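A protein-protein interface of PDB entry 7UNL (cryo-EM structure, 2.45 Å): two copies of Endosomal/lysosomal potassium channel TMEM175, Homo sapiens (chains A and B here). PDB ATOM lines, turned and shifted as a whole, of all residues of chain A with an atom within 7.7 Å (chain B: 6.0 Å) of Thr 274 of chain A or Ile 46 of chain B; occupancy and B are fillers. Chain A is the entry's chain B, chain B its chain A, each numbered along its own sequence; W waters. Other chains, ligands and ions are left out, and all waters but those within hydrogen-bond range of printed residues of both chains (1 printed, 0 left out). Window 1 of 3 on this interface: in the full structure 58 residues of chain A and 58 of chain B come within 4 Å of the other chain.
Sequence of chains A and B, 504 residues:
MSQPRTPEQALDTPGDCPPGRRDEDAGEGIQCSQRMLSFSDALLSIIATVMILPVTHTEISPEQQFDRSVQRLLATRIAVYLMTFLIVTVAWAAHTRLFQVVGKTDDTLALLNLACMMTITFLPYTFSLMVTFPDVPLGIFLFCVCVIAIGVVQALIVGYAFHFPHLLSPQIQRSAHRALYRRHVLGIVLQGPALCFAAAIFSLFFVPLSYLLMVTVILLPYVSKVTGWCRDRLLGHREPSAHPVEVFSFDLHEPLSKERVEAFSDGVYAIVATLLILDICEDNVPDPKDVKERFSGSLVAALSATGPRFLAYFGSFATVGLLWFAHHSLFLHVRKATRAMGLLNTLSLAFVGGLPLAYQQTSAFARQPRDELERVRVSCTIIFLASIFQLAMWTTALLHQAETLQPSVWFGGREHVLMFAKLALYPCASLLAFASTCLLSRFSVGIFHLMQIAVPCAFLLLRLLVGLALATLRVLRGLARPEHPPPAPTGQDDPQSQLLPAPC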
ATOM      1  N   ILE A  46      16.534 -13.333  18.737  1.00  0.00           N
ATOM      2  CA  ILE A  46      17.716 -13.504  19.577  1.00  0.00           C
ATOM      3  C   ILE A  46      18.988 -13.295  18.760  1.00  0.00           C
ATOM      4  O   ILE A  46      19.919 -12.612  19.203  1.00  0.00           O
ATOM      5  CB  ILE A  46      17.705 -14.882  20.258  1.00  0.00           C
ATOM      6  CG1 ILE A  46      16.586 -14.945  21.293  1.00  0.00           C
ATOM      7  CG2 ILE A  46      19.045 -15.159  20.920  1.00  0.00           C
ATOM      8  CD1 ILE A  46      16.278 -16.336  21.773  1.00  0.00           C
ATOM      9  N   ASP A 266       8.273  -7.934  18.936  1.00  0.00           N
ATOM     10  CA  ASP A 266       8.060  -8.233  20.348  1.00  0.00           C
ATOM     11  C   ASP A 266       9.298  -8.868  20.965  1.00  0.00           C
ATOM     12  O   ASP A 266       9.713  -8.504  22.073  1.00  0.00           O
ATOM     13  CB  ASP A 266       6.852  -9.160  20.502  1.00  0.00           C
ATOM     14  CG  ASP A 266       5.555  -8.406  20.709  1.00  0.00           C
ATOM     15  OD1 ASP A 266       5.592  -7.173  20.881  1.00  0.00           O
ATOM     16  OD2 ASP A 266       4.489  -9.055  20.693  1.00  0.00           O
ATOM     17  N   GLY A 267       9.897  -9.831  20.264  1.00  0.00           N
ATOM     18  CA  GLY A 267      11.109 -10.449  20.776  1.00  0.00           C
ATOM     19  C   GLY A 267      12.240  -9.455  20.953  1.00  0.00           C
ATOM     20  O   GLY A 267      12.915  -9.439  21.992  1.00  0.00           O
ATOM     21  N   VAL A 268      12.458  -8.605  19.947  1.00  0.00           N
ATOM     22  CA  VAL A 268      13.518  -7.603  20.045  1.00  0.00           C
ATOM     23  C   VAL A 268      13.260  -6.677  21.229  1.00  0.00           C
ATOM     24  O   VAL A 268      14.170  -6.363  22.007  1.00  0.00           O
ATOM     25  CB  VAL A 268      13.639  -6.817  18.726  1.00  0.00           C
ATOM     26  CG1 VAL A 268      14.571  -5.622  18.890  1.00  0.00           C
ATOM     27  CG2 VAL A 268      14.130  -7.721  17.610  1.00  0.00           C
ATOM     28  N   TYR A 269      12.012  -6.227  21.382  1.00  0.00           N
ATOM     29  CA  TYR A 269      11.678  -5.313  22.468  1.00  0.00           C
ATOM     30  C   TYR A 269      11.927  -5.956  23.826  1.00  0.00           C
ATOM     31  O   TYR A 269      12.478  -5.317  24.727  1.00  0.00           O
ATOM     32  CB  TYR A 269      10.221  -4.865  22.353  1.00  0.00           C
ATOM     33  CG  TYR A 269       9.987  -3.686  21.436  1.00  0.00           C
ATOM     34  CD1 TYR A 269      10.539  -2.445  21.705  1.00  0.00           C
ATOM     35  CD2 TYR A 269       9.192  -3.814  20.308  1.00  0.00           C
ATOM     36  CE1 TYR A 269      10.319  -1.374  20.873  1.00  0.00           C
ATOM     37  CE2 TYR A 269       8.967  -2.750  19.472  1.00  0.00           C
ATOM     38  CZ  TYR A 269       9.532  -1.531  19.757  1.00  0.00           C
ATOM     39  OH  TYR A 269       9.309  -0.465  18.923  1.00  0.00           O
ATOM     40  N   ALA A 270      11.525  -7.218  23.994  1.00  0.00           N
ATOM     41  CA  ALA A 270      11.735  -7.893  25.271  1.00  0.00           C
ATOM     42  C   ALA A 270      13.222  -8.019  25.587  1.00  0.00           C
ATOM     43  O   ALA A 270      13.658  -7.751  26.717  1.00  0.00           O
ATOM     44  CB  ALA A 270      11.062  -9.266  25.253  1.00  0.00           C
ATOM     45  N   ILE A 271      14.021  -8.417  24.593  1.00  0.00           N
ATOM     46  CA  ILE A 271      15.458  -8.556  24.819  1.00  0.00           C
ATOM     47  C   ILE A 271      16.064  -7.219  25.233  1.00  0.00           C
ATOM     48  O   ILE A 271      16.849  -7.137  26.188  1.00  0.00           O
ATOM     49  CB  ILE A 271      16.147  -9.122  23.564  1.00  0.00           C
ATOM     50  CG1 ILE A 271      15.725 -10.573  23.339  1.00  0.00           C
ATOM     51  CG2 ILE A 271      17.655  -9.020  23.690  1.00  0.00           C
ATOM     52  CD1 ILE A 271      15.886 -11.042  21.917  1.00  0.00           C
ATOM     53  N   VAL A 272      15.713  -6.150  24.514  1.00  0.00           N
ATOM     54  CA  VAL A 272      16.307  -4.849  24.798  1.00  0.00           C
ATOM     55  C   VAL A 272      15.865  -4.348  26.166  1.00  0.00           C
ATOM     56  O   VAL A 272      16.639  -3.705  26.886  1.00  0.00           O
ATOM     57  CB  VAL A 272      15.958  -3.851  23.679  1.00  0.00           C
ATOM     58  CG1 VAL A 272      16.489  -2.469  24.005  1.00  0.00           C
ATOM     59  CG2 VAL A 272      16.529  -4.326  22.358  1.00  0.00           C
ATOM     60  N   ALA A 273      14.619  -4.631  26.549  1.00  0.00           N
ATOM     61  CA  ALA A 273      14.128  -4.187  27.846  1.00  0.00           C
ATOM     62  C   ALA A 273      14.794  -4.931  28.998  1.00  0.00           C
ATOM     63  O   ALA A 273      14.978  -4.350  30.074  1.00  0.00           O
ATOM     64  CB  ALA A 273      12.610  -4.354  27.912  1.00  0.00           C
ATOM     65  N   THR A 274      15.153  -6.203  28.810  1.00  0.00           N
ATOM     66  CA  THR A 274      15.721  -6.999  29.896  1.00  0.00           C
ATOM     67  C   THR A 274      17.242  -7.121  29.862  1.00  0.00           C
ATOM     68  O   THR A 274      17.813  -7.803  30.727  1.00  0.00           O
ATOM     69  CB  THR A 274      15.101  -8.402  29.894  1.00  0.00           C
ATOM     70  OG1 THR A 274      15.300  -9.019  28.618  1.00  0.00           O
ATOM     71  CG2 THR A 274      13.620  -8.322  30.199  1.00  0.00           C
ATOM     72  N   LEU A 275      17.915  -6.493  28.896  1.00  0.00           N
ATOM     73  CA  LEU A 275      19.376  -6.572  28.837  1.00  0.00           C
ATOM     74  C   LEU A 275      20.024  -6.186  30.167  1.00  0.00           C
ATOM     75  O   LEU A 275      20.852  -6.929  30.718  1.00  0.00           O
ATOM     76  CB  LEU A 275      19.890  -5.654  27.728  1.00  0.00           C
ATOM     77  CG  LEU A 275      20.056  -6.174  26.300  1.00  0.00           C
ATOM     78  CD1 LEU A 275      20.766  -5.122  25.468  1.00  0.00           C
ATOM     79  CD2 LEU A 275      20.817  -7.479  26.259  1.00  0.00           C
ATOM     80  N   LEU A 276      19.660  -5.016  30.696  1.00  0.00           N
ATOM     81  CA  LEU A 276      20.370  -4.483  31.852  1.00  0.00           C
ATOM     82  C   LEU A 276      20.071  -5.285  33.111  1.00  0.00           C
ATOM     83  O   LEU A 276      20.949  -5.453  33.962  1.00  0.00           O
ATOM     84  CB  LEU A 276      20.018  -3.010  32.054  1.00  0.00           C
ATOM     85  CG  LEU A 276      20.510  -2.030  30.982  1.00  0.00           C
ATOM     86  CD1 LEU A 276      20.250  -0.607  31.424  1.00  0.00           C
ATOM     87  CD2 LEU A 276      21.983  -2.226  30.671  1.00  0.00           C
ATOM     88  N   ILE A 277      18.843  -5.785  33.256  1.00  0.00           N
ATOM     89  CA  ILE A 277      18.540  -6.609  34.422  1.00  0.00           C
ATOM     90  C   ILE A 277      19.272  -7.940  34.339  1.00  0.00           C
ATOM     91  O   ILE A 277      19.713  -8.481  35.357  1.00  0.00           O
ATOM     92  CB  ILE A 277      17.019  -6.795  34.587  1.00  0.00           C
ATOM     93  CG1 ILE A 277      16.690  -7.323  35.986  1.00  0.00           C
ATOM     94  CG2 ILE A 277      16.449  -7.720  33.528  1.00  0.00           C
ATOM     95  CD1 ILE A 277      17.130  -6.422  37.114  1.00  0.00           C
ATOM     96  N   LEU A 278      19.416  -8.495  33.133  1.00  0.00           N
ATOM     97  CA  LEU A 278      20.232  -9.698  32.989  1.00  0.00           C
ATOM     98  C   LEU A 278      21.661  -9.434  33.453  1.00  0.00           C
ATOM     99  O   LEU A 278      22.237 -10.213  34.230  1.00  0.00           O
ATOM    100  CB  LEU A 278      20.214 -10.166  31.533  1.00  0.00           C
ATOM    101  CG  LEU A 278      19.260 -11.305  31.173  1.00  0.00           C
ATOM    102  CD1 LEU A 278      17.812 -10.890  31.364  1.00  0.00           C
ATOM    103  CD2 LEU A 278      19.502 -11.748  29.747  1.00  0.00           C
ATOM    104  N   ASP A 279      22.238  -8.318  33.005  1.00  0.00           N
ATOM    105  CA  ASP A 279      23.602  -7.989  33.409  1.00  0.00           C
ATOM    106  C   ASP A 279      23.701  -7.780  34.917  1.00  0.00           C
ATOM    107  O   ASP A 279      24.673  -8.213  35.548  1.00  0.00           O
ATOM    108  CB  ASP A 279      24.089  -6.748  32.664  1.00  0.00           C
ATOM    109  CG  ASP A 279      25.530  -6.869  32.212  1.00  0.00           C
ATOM    110  OD1 ASP A 279      25.901  -7.937  31.680  1.00  0.00           O
ATOM    111  OD2 ASP A 279      26.295  -5.897  32.389  1.00  0.00           O
ATOM    112  N   ILE A 280      22.712  -7.109  35.512  1.00  0.00           N
ATOM    113  CA  ILE A 280      22.720  -6.890  36.955  1.00  0.00           C
ATOM    114  C   ILE A 280      22.655  -8.214  37.700  1.00  0.00           C
ATOM    115  O   ILE A 280      23.419  -8.450  38.642  1.00  0.00           O
ATOM    116  CB  ILE A 280      21.557  -5.965  37.360  1.00  0.00           C
ATOM    117  CG1 ILE A 280      21.838  -4.530  36.920  1.00  0.00           C
ATOM    118  CG2 ILE A 280      21.319  -6.034  38.863  1.00  0.00           C
ATOM    119  CD1 ILE A 280      20.653  -3.607  37.058  1.00  0.00           C
ATOM    120  N   CYS A 281      21.741  -9.096  37.297  1.00  0.00           N
ATOM    121  CA  CYS A 281      21.596 -10.381  37.958  1.00  0.00           C
ATOM    122  C   CYS A 281      22.846 -11.235  37.841  1.00  0.00           C
ATOM    123  O   CYS A 281      23.112 -12.037  38.742  1.00  0.00           O
ATOM    124  CB  CYS A 281      20.401 -11.139  37.380  1.00  0.00           C
ATOM    125  SG  CYS A 281      18.811 -10.327  37.632  1.00  0.00           S
ATOM    126  N   TYR A 313      18.378   0.669  34.447  1.00  0.00           N
ATOM    127  CA  TYR A 313      17.430  -0.368  34.046  1.00  0.00           C
ATOM    128  C   TYR A 313      15.997   0.153  34.083  1.00  0.00           C
ATOM    129  O   TYR A 313      15.219  -0.060  33.149  1.00  0.00           O
ATOM    130  CB  TYR A 313      17.558  -1.590  34.951  1.00  0.00           C
ATOM    131  CG  TYR A 313      16.475  -2.604  34.682  1.00  0.00           C
ATOM    132  CD1 TYR A 313      16.306  -3.145  33.418  1.00  0.00           C
ATOM    133  CD2 TYR A 313      15.599  -2.993  35.684  1.00  0.00           C
ATOM    134  CE1 TYR A 313      15.311  -4.053  33.161  1.00  0.00           C
ATOM    135  CE2 TYR A 313      14.600  -3.903  35.435  1.00  0.00           C
ATOM    136  CZ  TYR A 313      14.457  -4.429  34.173  1.00  0.00           C
ATOM    137  OH  TYR A 313      13.461  -5.340  33.923  1.00  0.00           O
ATOM    138  N   SER A 316      15.592   2.444  31.018  1.00  0.00           N
ATOM    139  CA  SER A 316      15.611   1.701  29.765  1.00  0.00           C
ATOM    140  C   SER A 316      14.340   0.882  29.591  1.00  0.00           C
ATOM    141  O   SER A 316      13.725   0.883  28.521  1.00  0.00           O
ATOM    142  CB  SER A 316      16.844   0.797  29.727  1.00  0.00           C
ATOM    143  OG  SER A 316      17.303   0.604  28.407  1.00  0.00           O
ATOM    144  N   PHE A 317      13.945   0.154  30.635  1.00  0.00           N
ATOM    145  CA  PHE A 317      12.744  -0.666  30.563  1.00  0.00           C
ATOM    146  C   PHE A 317      11.515   0.196  30.341  1.00  0.00           C
ATOM    147  O   PHE A 317      10.656  -0.140  29.524  1.00  0.00           O
ATOM    148  CB  PHE A 317      12.602  -1.496  31.839  1.00  0.00           C
ATOM    149  CG  PHE A 317      11.466  -2.480  31.809  1.00  0.00           C
ATOM    150  CD1 PHE A 317      10.163  -2.072  32.039  1.00  0.00           C
ATOM    151  CD2 PHE A 317      11.701  -3.816  31.541  1.00  0.00           C
ATOM    152  CE1 PHE A 317       9.127  -2.976  32.009  1.00  0.00           C
ATOM    153  CE2 PHE A 317      10.666  -4.722  31.509  1.00  0.00           C
ATOM    154  CZ  PHE A 317       9.377  -4.302  31.744  1.00  0.00           C
ATOM    155  N   VAL A 320      11.640   1.476  26.615  1.00  0.00           N
ATOM    156  CA  VAL A 320      11.422   0.397  25.655  1.00  0.00           C
ATOM    157  C   VAL A 320       9.983  -0.091  25.729  1.00  0.00           C
ATOM    158  O   VAL A 320       9.349  -0.363  24.704  1.00  0.00           O
ATOM    159  CB  VAL A 320      12.423  -0.749  25.893  1.00  0.00           C
ATOM    160  CG1 VAL A 320      12.140  -1.915  24.961  1.00  0.00           C
ATOM    161  CG2 VAL A 320      13.845  -0.265  25.696  1.00  0.00           C
ATOM    162  N   PRO A 356      19.594   0.917  25.961  1.00  0.00           N
ATOM    163  CA  PRO A 356      20.287   0.551  27.207  1.00  0.00           C
ATOM    164  C   PRO A 356      21.654   1.197  27.340  1.00  0.00           C
ATOM    165  O   PRO A 356      22.030   1.617  28.439  1.00  0.00           O
ATOM    166  CB  PRO A 356      20.373  -0.978  27.113  1.00  0.00           C
ATOM    167  CG  PRO A 356      19.238  -1.354  26.253  1.00  0.00           C
ATOM    168  CD  PRO A 356      19.150  -0.278  25.225  1.00  0.00           C
ATOM    169  N   ASP B  41       4.686 -13.202  27.753  1.00  0.00           N
ATOM    170  CA  ASP B  41       5.290 -14.528  27.775  1.00  0.00           C
ATOM    171  C   ASP B  41       6.765 -14.466  27.409  1.00  0.00           C
ATOM    172  O   ASP B  41       7.594 -15.141  28.029  1.00  0.00           O
ATOM    173  CB  ASP B  41       4.543 -15.464  26.825  1.00  0.00           C
ATOM    174  CG  ASP B  41       3.397 -16.188  27.495  1.00  0.00           C
ATOM    175  OD1 ASP B  41       3.446 -16.386  28.726  1.00  0.00           O
ATOM    176  OD2 ASP B  41       2.439 -16.558  26.787  1.00  0.00           O
ATOM    177  N   ALA B  42       7.112 -13.669  26.398  1.00  0.00           N
ATOM    178  CA  ALA B  42       8.520 -13.524  26.033  1.00  0.00           C
ATOM    179  C   ALA B  42       9.335 -12.946  27.186  1.00  0.00           C
ATOM    180  O   ALA B  42      10.414 -13.461  27.519  1.00  0.00           O
ATOM    181  CB  ALA B  42       8.647 -12.648  24.789  1.00  0.00           C
ATOM    182  N   LEU B  43       8.832 -11.883  27.819  1.00  0.00           N
ATOM    183  CA  LEU B  43       9.547 -11.306  28.954  1.00  0.00           C
ATOM    184  C   LEU B  43       9.715 -12.326  30.075  1.00  0.00           C
ATOM    185  O   LEU B  43      10.811 -12.484  30.627  1.00  0.00           O
ATOM    186  CB  LEU B  43       8.817 -10.066  29.470  1.00  0.00           C
ATOM    187  CG  LEU B  43       8.928  -8.792  28.633  1.00  0.00           C
ATOM    188  CD1 LEU B  43       7.827  -7.822  29.008  1.00  0.00           C
ATOM    189  CD2 LEU B  43      10.292  -8.150  28.809  1.00  0.00           C
ATOM    190  N   LEU B  44       8.638 -13.033  30.419  1.00  0.00           N
ATOM    191  CA  LEU B  44       8.697 -13.995  31.513  1.00  0.00           C
ATOM    192  C   LEU B  44       9.667 -15.127  31.200  1.00  0.00           C
ATOM    193  O   LEU B  44      10.391 -15.595  32.085  1.00  0.00           O
ATOM    194  CB  LEU B  44       7.298 -14.540  31.800  1.00  0.00           C
ATOM    195  CG  LEU B  44       6.390 -13.588  32.584  1.00  0.00           C
ATOM    196  CD1 LEU B  44       4.925 -13.950  32.414  1.00  0.00           C
ATOM    197  CD2 LEU B  44       6.770 -13.577  34.053  1.00  0.00           C
ATOM    198  N   SER B  45       9.693 -15.582  29.947  1.00  0.00           N
ATOM    199  CA  SER B  45      10.654 -16.604  29.554  1.00  0.00           C
ATOM    200  C   SER B  45      12.083 -16.107  29.701  1.00  0.00           C
ATOM    201  O   SER B  45      12.960 -16.868  30.126  1.00  0.00           O
ATOM    202  CB  SER B  45      10.391 -17.051  28.116  1.00  0.00           C
ATOM    203  OG  SER B  45      10.665 -16.013  27.194  1.00  0.00           O
ATOM    204  N   ILE B  46      12.346 -14.847  29.351  1.00  0.00           N
ATOM    205  CA  ILE B  46      13.685 -14.306  29.560  1.00  0.00           C
ATOM    206  C   ILE B  46      14.028 -14.277  31.045  1.00  0.00           C
ATOM    207  O   ILE B  46      15.132 -14.661  31.450  1.00  0.00           O
ATOM    208  CB  ILE B  46      13.814 -12.910  28.927  1.00  0.00           C
ATOM    209  CG1 ILE B  46      13.763 -13.018  27.405  1.00  0.00           C
ATOM    210  CG2 ILE B  46      15.111 -12.246  29.360  1.00  0.00           C
ATOM    211  CD1 ILE B  46      13.547 -11.704  26.708  1.00  0.00           C
ATOM    212  N   ILE B  47      13.093 -13.822  31.882  1.00  0.00           N
ATOM    213  CA  ILE B  47      13.379 -13.681  33.308  1.00  0.00           C
ATOM    214  C   ILE B  47      13.557 -15.045  33.966  1.00  0.00           C
ATOM    215  O   ILE B  47      14.394 -15.211  34.860  1.00  0.00           O
ATOM    216  CB  ILE B  47      12.269 -12.859  33.991  1.00  0.00           C
ATOM    217  CG1 ILE B  47      12.194 -11.455  33.386  1.00  0.00           C
ATOM    218  CG2 ILE B  47      12.495 -12.776  35.492  1.00  0.00           C
ATOM    219  CD1 ILE B  47      13.490 -10.667  33.456  1.00  0.00           C
ATOM    220  N   ALA B  48      12.774 -16.041  33.547  1.00  0.00           N
ATOM    221  CA  ALA B  48      12.872 -17.367  34.146  1.00  0.00           C
ATOM    222  C   ALA B  48      14.222 -18.025  33.893  1.00  0.00           C
ATOM    223  O   ALA B  48      14.622 -18.904  34.663  1.00  0.00           O
ATOM    224  CB  ALA B  48      11.755 -18.263  33.614  1.00  0.00           C
ATOM    225  N   THR B  49      14.931 -17.622  32.841  1.00  0.00           N
ATOM    226  CA  THR B  49      16.203 -18.225  32.468  1.00  0.00           C
ATOM    227  C   THR B  49      17.407 -17.357  32.810  1.00  0.00           C
ATOM    228  O   THR B  49      18.516 -17.664  32.363  1.00  0.00           O
ATOM    229  CB  THR B  49      16.216 -18.538  30.967  1.00  0.00           C
ATOM    230  OG1 THR B  49      15.810 -17.381  30.227  1.00  0.00           O
ATOM    231  CG2 THR B  49      15.282 -19.690  30.648  1.00  0.00           C
ATOM    232  N   VAL B  50      17.229 -16.290  33.591  1.00  0.00           N
ATOM    233  CA  VAL B  50      18.334 -15.373  33.866  1.00  0.00           C
ATOM    234  C   VAL B  50      19.447 -16.086  34.626  1.00  0.00           C
ATOM    235  O   VAL B  50      20.637 -15.865  34.375  1.00  0.00           O
ATOM    236  CB  VAL B  50      17.829 -14.135  34.630  1.00  0.00           C
ATOM    237  CG1 VAL B  50      17.442 -14.491  36.051  1.00  0.00           C
ATOM    238  CG2 VAL B  50      18.890 -13.050  34.633  1.00  0.00           C
ATOM    239  N   THR B 121      10.431  -8.847  37.068  1.00  0.00           N
ATOM    240  CA  THR B 121      11.829  -8.942  36.657  1.00  0.00           C
ATOM    241  C   THR B 121      12.806  -8.902  37.826  1.00  0.00           C
ATOM    242  O   THR B 121      13.968  -9.282  37.644  1.00  0.00           O
ATOM    243  CB  THR B 121      12.183  -7.821  35.675  1.00  0.00           C
ATOM    244  OG1 THR B 121      12.101  -6.549  36.333  1.00  0.00           O
ATOM    245  CG2 THR B 121      11.271  -7.849  34.466  1.00  0.00           C
ATOM    246  N   ILE B 271      15.932 -19.605  23.942  1.00  0.00           N
ATOM    247  CA  ILE B 271      17.025 -19.095  24.766  1.00  0.00           C
ATOM    248  C   ILE B 271      18.050 -20.192  25.030  1.00  0.00           C
ATOM    249  O   ILE B 271      19.265 -19.981  24.905  1.00  0.00           O
ATOM    250  CB  ILE B 271      16.478 -18.508  26.080  1.00  0.00           C
ATOM    251  CG1 ILE B 271      15.680 -17.236  25.798  1.00  0.00           C
ATOM    252  CG2 ILE B 271      17.608 -18.222  27.051  1.00  0.00           C
ATOM    253  CD1 ILE B 271      14.683 -16.889  26.873  1.00  0.00           C
HETATM  254  O   HOH W   1      15.999 -10.119  38.630  1.00  0.00           O
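Water W1 lies within hydrogen-bond range of O of Thr 121 of chain B (2.4 Å) and SG of Cys 281 of chain A (3.0 Å).
The side-chain hydroxyl (OG1) of Thr 49 of chain B lies within hydrogen-bond range of the backbone carbonyl oxygen (O) of Ile 46 of chain B (3.1 Å).
O of Ala 270 of chain A is in hydrogen-bond range of OG1 of Thr 274 of chain A, 2.8 Å away.
O of Ile 271 of chain A is in hydrogen-bond range of OG1 of Thr 274 of chain A, 3.4 Å away.
O of Ile 277 of chain A lies within hydrogen-bond range of SG of Cys 281 of chain A (3.1 Å).
The side-chain hydroxyl (OH) of Tyr 313 of chain A lies within hydrogen-bond range of the side-chain hydroxyl (OG1) of Thr 121 of chain B (3.0 Å).
Among the printed residues, pairs that only touch across the chains: Ile 46 of chain A with Ile 271 of chain B, Ala 270 of chain A with Leu 43 of chain B, Ala 270 of chain A with Ile 46 of chain B, Ile 271 of chain A with Ile 46 of chain B, Thr 274 of chain A with Leu 43 of chain B, Thr 274 of chain A with Ile 46 of chain B, Ile 277 of chain A with Thr 121 of chain B, Leu 278 of chain A with Ile 46 of chain B, Leu 278 of chain A with Val 50 of chain B and Cys 281 of chain A with Val 50 of chain B.
Of the 22 printed residues of chain A, 8 touch a printed residue of chain B.
Printed residues of chain A that touch a printed residue of chain B: Ile 46, Ala 270, Ile 271, Thr 274, Ile 277, Leu 278, Cys 281 and Tyr 313.
Printed residues of chain B that touch a printed residue of chain A: Leu 43, Ile 46, Val 50, Thr 121 and Ile 271.
Among the printed residues, no Asp or Glu carboxylate lies within 4 Å of a Lys or Arg side-chain nitrogen of the other chain.
Ile 46 of chain A touches Ile 271 of chain B, and with the chains exchanged Ile 271 of chain A touches Ile 46 of chain B.
Of the 11 pairs that touch across the chains among the printed residues, 2 have their exchanged pair printed and touching as well.
Printed residues of chain B within 4 Å of Thr 274 of chain A: Leu 43 (3.6 Å) and Ile 46 (3.3 Å).
Ile 46 of chain B touches four residues of chain A.
No residue of chain A comes within 4 Å of Ser 45 of chain B.
Printed residues of chain A within 4 Å of Thr 121 of chain B: Ile 277 and Tyr 313.
Of the printed residues of chain B, Tyr 313 of chain A touches Thr 121.
Printed residues of chain A within 4 Å of Leu 43 of chain B: Ala 270 (3.8 Å) and Thr 274 (3.6 Å).
Of the printed residues of chain B, Ile 277 of chain A touches Thr 121 (3.7 Å).
Tyr 269 of chain A touches none of the printed residues of chain B.
The nearest printed residue of chain B that does not touch Thr 274 of chain A is Ile 47 of chain B (4.02 Å).
The nearest residue of chain A that does not touch Ile 46 of chain B is Gly 267 of chain A (5.3 Å).
The nearest printed residue of chain B that does not touch Leu 278 of chain A is Ile 47 of chain B (4.8 Å).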
